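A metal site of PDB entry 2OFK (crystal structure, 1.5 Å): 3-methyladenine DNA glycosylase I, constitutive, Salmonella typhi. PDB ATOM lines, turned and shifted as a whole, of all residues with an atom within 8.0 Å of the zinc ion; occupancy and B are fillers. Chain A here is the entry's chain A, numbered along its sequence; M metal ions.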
ATOM      1  N   GLN A   2     -23.531  -3.586  -9.027  1.00  0.00           N
ATOM      2  CA  GLN A   2     -24.192  -3.786  -7.698  1.00  0.00           C
ATOM      3  C   GLN A   2     -24.535  -2.439  -7.070  1.00  0.00           C
ATOM      4  O   GLN A   2     -23.816  -1.470  -7.257  1.00  0.00           O
ATOM      5  CB  GLN A   2     -23.301  -4.597  -6.748  1.00  0.00           C
ATOM      6  N   ARG A   3     -25.630  -2.415  -6.311  1.00  0.00           N
ATOM      7  CA  ARG A   3     -26.044  -1.229  -5.561  1.00  0.00           C
ATOM      8  C   ARG A   3     -26.111  -1.579  -4.088  1.00  0.00           C
ATOM      9  O   ARG A   3     -26.190  -2.760  -3.741  1.00  0.00           O
ATOM     10  CB  ARG A   3     -27.454  -0.774  -5.959  1.00  0.00           C
ATOM     11  CG  ARG A   3     -27.525  -0.083  -7.282  1.00  0.00           C
ATOM     12  CD  ARG A   3     -28.916   0.437  -7.568  1.00  0.00           C
ATOM     13  NE  ARG A   3     -28.865   1.211  -8.797  1.00  0.00           N
ATOM     14  CZ  ARG A   3     -29.028   0.687 -10.017  1.00  0.00           C
ATOM     15  NH1 ARG A   3     -29.312  -0.607 -10.168  1.00  0.00           N
ATOM     16  NH2 ARG A   3     -28.936   1.472 -11.082  1.00  0.00           N
ATOM     17  N   CYS A   4     -26.139  -0.573  -3.233  1.00  0.00           N
ATOM     18  CA  CYS A   4     -26.481  -0.816  -1.820  1.00  0.00           C
ATOM     19  C   CYS A   4     -27.727  -1.687  -1.669  1.00  0.00           C
ATOM     20  O   CYS A   4     -28.685  -1.558  -2.411  1.00  0.00           O
ATOM     21  CB  CYS A   4     -26.696   0.488  -1.115  1.00  0.00           C
ATOM     22  SG  CYS A   4     -25.143   1.401  -0.886  1.00  0.00           S
ATOM     23  N   ASP A   5     -27.703  -2.553  -0.676  1.00  0.00           N
ATOM     24  CA  ASP A   5     -28.726  -3.575  -0.488  1.00  0.00           C
ATOM     25  C   ASP A   5     -30.092  -2.977  -0.062  1.00  0.00           C
ATOM     26  O   ASP A   5     -31.131  -3.564  -0.319  1.00  0.00           O
ATOM     27  CB  ASP A   5     -28.246  -4.581   0.565  1.00  0.00           C
ATOM     28  CG  ASP A   5     -29.121  -5.816   0.649  1.00  0.00           C
ATOM     29  OD1 ASP A   5     -29.574  -6.329  -0.418  1.00  0.00           O
ATOM     30  OD2 ASP A   5     -29.339  -6.269   1.791  1.00  0.00           O
ATOM     31  N   TRP A   6     -30.066  -1.817   0.601  1.00  0.00           N
ATOM     32  CA  TRP A   6     -31.302  -1.199   1.071  1.00  0.00           C
ATOM     33  C   TRP A   6     -32.194  -0.569   0.006  1.00  0.00           C
ATOM     34  O   TRP A   6     -33.349  -0.226   0.298  1.00  0.00           O
ATOM     35  CB  TRP A   6     -31.004  -0.174   2.181  1.00  0.00           C
ATOM     36  CG  TRP A   6     -29.952   0.831   1.841  1.00  0.00           C
ATOM     37  CD1 TRP A   6     -28.646   0.808   2.233  1.00  0.00           C
ATOM     38  CD2 TRP A   6     -30.114   2.017   1.035  1.00  0.00           C
ATOM     39  NE1 TRP A   6     -27.990   1.890   1.757  1.00  0.00           N
ATOM     40  CE2 TRP A   6     -28.848   2.657   1.002  1.00  0.00           C
ATOM     41  CE3 TRP A   6     -31.203   2.605   0.390  1.00  0.00           C
ATOM     42  CZ2 TRP A   6     -28.639   3.847   0.326  1.00  0.00           C
ATOM     43  CZ3 TRP A   6     -30.987   3.807  -0.356  1.00  0.00           C
ATOM     44  CH2 TRP A   6     -29.705   4.411  -0.359  1.00  0.00           C
ATOM     45  N   VAL A   7     -31.677  -0.385  -1.222  1.00  0.00           N
ATOM     46  CA  VAL A   7     -32.491   0.151  -2.309  1.00  0.00           C
ATOM     47  C   VAL A   7     -33.520  -0.900  -2.755  1.00  0.00           C
ATOM     48  O   VAL A   7     -33.227  -2.073  -2.776  1.00  0.00           O
ATOM     49  CB  VAL A   7     -31.584   0.551  -3.516  1.00  0.00           C
ATOM     50  CG1 VAL A   7     -32.378   1.420  -4.542  1.00  0.00           C
ATOM     51  CG2 VAL A   7     -30.392   1.311  -3.034  1.00  0.00           C
ATOM     52  N   HIS A  17     -30.995   6.763  -4.819  1.00  0.00           N
ATOM     53  CA  HIS A  17     -29.735   6.122  -4.415  1.00  0.00           C
ATOM     54  C   HIS A  17     -28.574   6.496  -5.364  1.00  0.00           C
ATOM     55  O   HIS A  17     -27.464   6.836  -4.923  1.00  0.00           O
ATOM     56  CB  HIS A  17     -29.856   4.604  -4.380  1.00  0.00           C
ATOM     57  CG  HIS A  17     -28.524   3.922  -4.330  1.00  0.00           C
ATOM     58  ND1 HIS A  17     -27.814   3.586  -5.464  1.00  0.00           N
ATOM     59  CD2 HIS A  17     -27.744   3.588  -3.275  1.00  0.00           C
ATOM     60  CE1 HIS A  17     -26.658   3.038  -5.099  1.00  0.00           C
ATOM     61  NE2 HIS A  17     -26.593   3.040  -3.782  1.00  0.00           N
ATOM     62  N   ASP A  18     -28.850   6.427  -6.674  1.00  0.00           N
ATOM     63  CA  ASP A  18     -27.795   6.541  -7.668  1.00  0.00           C
ATOM     64  C   ASP A  18     -27.340   7.972  -7.811  1.00  0.00           C
ATOM     65  O   ASP A  18     -26.156   8.223  -8.094  1.00  0.00           O
ATOM     66  CB  ASP A  18     -28.320   6.109  -9.031  1.00  0.00           C
ATOM     67  CG  ASP A  18     -28.490   4.625  -9.166  1.00  0.00           C
ATOM     68  OD1 ASP A  18     -28.270   3.865  -8.189  1.00  0.00           O
ATOM     69  OD2 ASP A  18     -28.869   4.229 -10.307  1.00  0.00           O
ATOM     70  N   TRP A  21     -28.136  10.226  -2.900  1.00  0.00           N
ATOM     71  CA  TRP A  21     -27.667   9.782  -1.569  1.00  0.00           C
ATOM     72  C   TRP A  21     -26.146   9.683  -1.503  1.00  0.00           C
ATOM     73  O   TRP A  21     -25.498   9.103  -2.377  1.00  0.00           O
ATOM     74  CB  TRP A  21     -28.276   8.422  -1.282  1.00  0.00           C
ATOM     75  CG  TRP A  21     -28.184   7.977   0.141  1.00  0.00           C
ATOM     76  CD1 TRP A  21     -29.008   8.336   1.146  1.00  0.00           C
ATOM     77  CD2 TRP A  21     -27.256   7.025   0.666  1.00  0.00           C
ATOM     78  NE1 TRP A  21     -28.613   7.701   2.328  1.00  0.00           N
ATOM     79  CE2 TRP A  21     -27.551   6.871   2.055  1.00  0.00           C
ATOM     80  CE3 TRP A  21     -26.197   6.295   0.121  1.00  0.00           C
ATOM     81  CZ2 TRP A  21     -26.850   5.984   2.889  1.00  0.00           C
ATOM     82  CZ3 TRP A  21     -25.489   5.426   0.939  1.00  0.00           C
ATOM     83  CH2 TRP A  21     -25.798   5.283   2.305  1.00  0.00           C
ATOM     84  N   ASN A 173     -20.060   9.161   3.532  1.00  0.00           N
ATOM     85  CA  ASN A 173     -20.379   8.382   2.338  1.00  0.00           C
ATOM     86  C   ASN A 173     -20.467   6.945   2.789  1.00  0.00           C
ATOM     87  O   ASN A 173     -19.440   6.289   3.000  1.00  0.00           O
ATOM     88  CB  ASN A 173     -19.284   8.549   1.281  1.00  0.00           C
ATOM     89  CG  ASN A 173     -19.591   7.823  -0.007  1.00  0.00           C
ATOM     90  OD1 ASN A 173     -20.331   6.830  -0.033  1.00  0.00           O
ATOM     91  ND2 ASN A 173     -18.999   8.288  -1.103  1.00  0.00           N
ATOM     92  N   ASP A 174     -21.706   6.455   2.941  1.00  0.00           N
ATOM     93  CA  ASP A 174     -21.923   5.103   3.481  1.00  0.00           C
ATOM     94  C   ASP A 174     -22.402   4.113   2.393  1.00  0.00           C
ATOM     95  O   ASP A 174     -23.021   3.095   2.700  1.00  0.00           O
ATOM     96  CB  ASP A 174     -22.919   5.107   4.672  1.00  0.00           C
ATOM     97  CG  ASP A 174     -22.258   5.479   6.005  1.00  0.00           C
ATOM     98  OD1 ASP A 174     -21.004   5.411   6.108  1.00  0.00           O
ATOM     99  OD2 ASP A 174     -23.019   5.734   7.004  1.00  0.00           O
ATOM    100  N   HIS A 175     -22.091   4.370   1.111  1.00  0.00           N
ATOM    101  CA  HIS A 175     -22.276   3.294   0.123  1.00  0.00           C
ATOM    102  C   HIS A 175     -21.358   2.151   0.508  1.00  0.00           C
ATOM    103  O   HIS A 175     -20.179   2.380   0.826  1.00  0.00           O
ATOM    104  CB  HIS A 175     -21.888   3.758  -1.260  1.00  0.00           C
ATOM    105  CG  HIS A 175     -22.825   4.763  -1.832  1.00  0.00           C
ATOM    106  ND1 HIS A 175     -24.013   4.407  -2.440  1.00  0.00           N
ATOM    107  CD2 HIS A 175     -22.771   6.108  -1.884  1.00  0.00           C
ATOM    108  CE1 HIS A 175     -24.631   5.492  -2.854  1.00  0.00           C
ATOM    109  NE2 HIS A 175     -23.895   6.539  -2.524  1.00  0.00           N
ATOM    110  N   ILE A 176     -21.849   0.918   0.449  1.00  0.00           N
ATOM    111  CA  ILE A 176     -20.983  -0.238   0.730  1.00  0.00           C
ATOM    112  C   ILE A 176     -19.890  -0.333  -0.349  1.00  0.00           C
ATOM    113  O   ILE A 176     -20.047   0.194  -1.451  1.00  0.00           O
ATOM    114  CB  ILE A 176     -21.788  -1.555   0.844  1.00  0.00           C
ATOM    115  CG1 ILE A 176     -22.650  -1.772  -0.401  1.00  0.00           C
ATOM    116  CG2 ILE A 176     -22.657  -1.503   2.125  1.00  0.00           C
ATOM    117  CD1 ILE A 176     -23.254  -3.184  -0.546  1.00  0.00           C
ATOM    118  N   THR A 177     -18.796  -1.000  -0.023  1.00  0.00           N
ATOM    119  CA  THR A 177     -17.614  -0.978  -0.905  1.00  0.00           C
ATOM    120  C   THR A 177     -17.897  -1.674  -2.213  1.00  0.00           C
ATOM    121  O   THR A 177     -17.254  -1.379  -3.224  1.00  0.00           O
ATOM    122  CB  THR A 177     -16.388  -1.624  -0.268  1.00  0.00           C
ATOM    123  OG1 THR A 177     -16.760  -2.914   0.223  1.00  0.00           O
ATOM    124  CG2 THR A 177     -15.875  -0.761   0.832  1.00  0.00           C
ATOM    125  N   GLY A 178     -18.861  -2.588  -2.201  1.00  0.00           N
ATOM    126  CA  GLY A 178     -19.292  -3.254  -3.424  1.00  0.00           C
ATOM    127  C   GLY A 178     -20.197  -2.436  -4.324  1.00  0.00           C
ATOM    128  O   GLY A 178     -20.368  -2.782  -5.497  1.00  0.00           O
ATOM    129  N   CYS A 179     -20.793  -1.357  -3.798  1.00  0.00           N
ATOM    130  CA  CYS A 179     -21.727  -0.541  -4.602  1.00  0.00           C
ATOM    131  C   CYS A 179     -20.959   0.252  -5.662  1.00  0.00           C
ATOM    132  O   CYS A 179     -19.895   0.797  -5.383  1.00  0.00           O
ATOM    133  CB  CYS A 179     -22.528   0.385  -3.678  1.00  0.00           C
ATOM    134  SG  CYS A 179     -23.607   1.540  -4.558  1.00  0.00           S
ATOM    135  N   PHE A 180     -21.524   0.319  -6.873  1.00  0.00           N
ATOM    136  CA  PHE A 180     -20.866   1.032  -7.970  1.00  0.00           C
ATOM    137  C   PHE A 180     -20.677   2.524  -7.648  1.00  0.00           C
ATOM    138  O   PHE A 180     -19.816   3.179  -8.255  1.00  0.00           O
ATOM    139  CB  PHE A 180     -21.646   0.836  -9.282  1.00  0.00           C
ATOM    140  CG  PHE A 180     -22.809   1.785  -9.468  1.00  0.00           C
ATOM    141  CD1 PHE A 180     -22.661   2.959 -10.197  1.00  0.00           C
ATOM    142  CD2 PHE A 180     -24.057   1.495  -8.915  1.00  0.00           C
ATOM    143  CE1 PHE A 180     -23.717   3.841 -10.371  1.00  0.00           C
ATOM    144  CE2 PHE A 180     -25.123   2.370  -9.082  1.00  0.00           C
ATOM    145  CZ  PHE A 180     -24.964   3.541  -9.798  1.00  0.00           C
ATOM    146  N   CYS A 181     -21.449   3.049  -6.705  1.00  0.00           N
ATOM    147  CA  CYS A 181     -21.318   4.439  -6.279  1.00  0.00           C
ATOM    148  C   CYS A 181     -20.205   4.659  -5.250  1.00  0.00           C
ATOM    149  O   CYS A 181     -19.909   5.804  -4.875  1.00  0.00           O
ATOM    150  CB  CYS A 181     -22.628   4.956  -5.700  1.00  0.00           C
ATOM    151  SG  CYS A 181     -23.971   5.116  -6.879  1.00  0.00           S
ATOM    152  N   HIS A 182     -19.599   3.586  -4.742  1.00  0.00           N
ATOM    153  CA  HIS A 182     -18.512   3.739  -3.775  1.00  0.00           C
ATOM    154  C   HIS A 182     -17.240   4.237  -4.499  1.00  0.00           C
ATOM    155  O   HIS A 182     -16.912   3.703  -5.554  1.00  0.00           O
ATOM    156  CB  HIS A 182     -18.256   2.429  -3.034  1.00  0.00           C
ATOM    157  CG  HIS A 182     -17.286   2.567  -1.906  1.00  0.00           C
ATOM    158  ND1 HIS A 182     -15.927   2.582  -2.096  1.00  0.00           N
ATOM    159  CD2 HIS A 182     -17.499   2.744  -0.585  1.00  0.00           C
ATOM    160  CE1 HIS A 182     -15.332   2.742  -0.924  1.00  0.00           C
ATOM    161  NE2 HIS A 182     -16.255   2.832   0.007  1.00  0.00           N
HETATM  162 ZN    ZN M   1     -24.793   2.566  -2.859  1.00  0.00          ZN
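The zinc ion is bound by a ring nitrogen (ND1) of His 175 (2.0 Å), a ring nitrogen (NE2) of His 17 (2.1 Å), the side-chain sulfur of Cys 179 (2.3 Å) and the side-chain sulfur of Cys 4 (2.3 Å).
The zinc ion has four donor atoms within binding distance.
ND1 of His 17 lies within hydrogen-bond range of OD1 of Asp 18, at 2.8 Å.
O of Trp 21 sits at hydrogen-bond distance from NE2 of His 175 (3.0 Å).
SG of Cys 4 lies close to N of Ile 176 (3.6 Å).
The side-chain sulfur (SG) of Cys 179 lies close to the backbone NH (N) of Cys 181 (3.4 Å).
The backbone NH of His 175 lies close to the side-chain amide oxygen of Asn 173 (3.2 Å).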
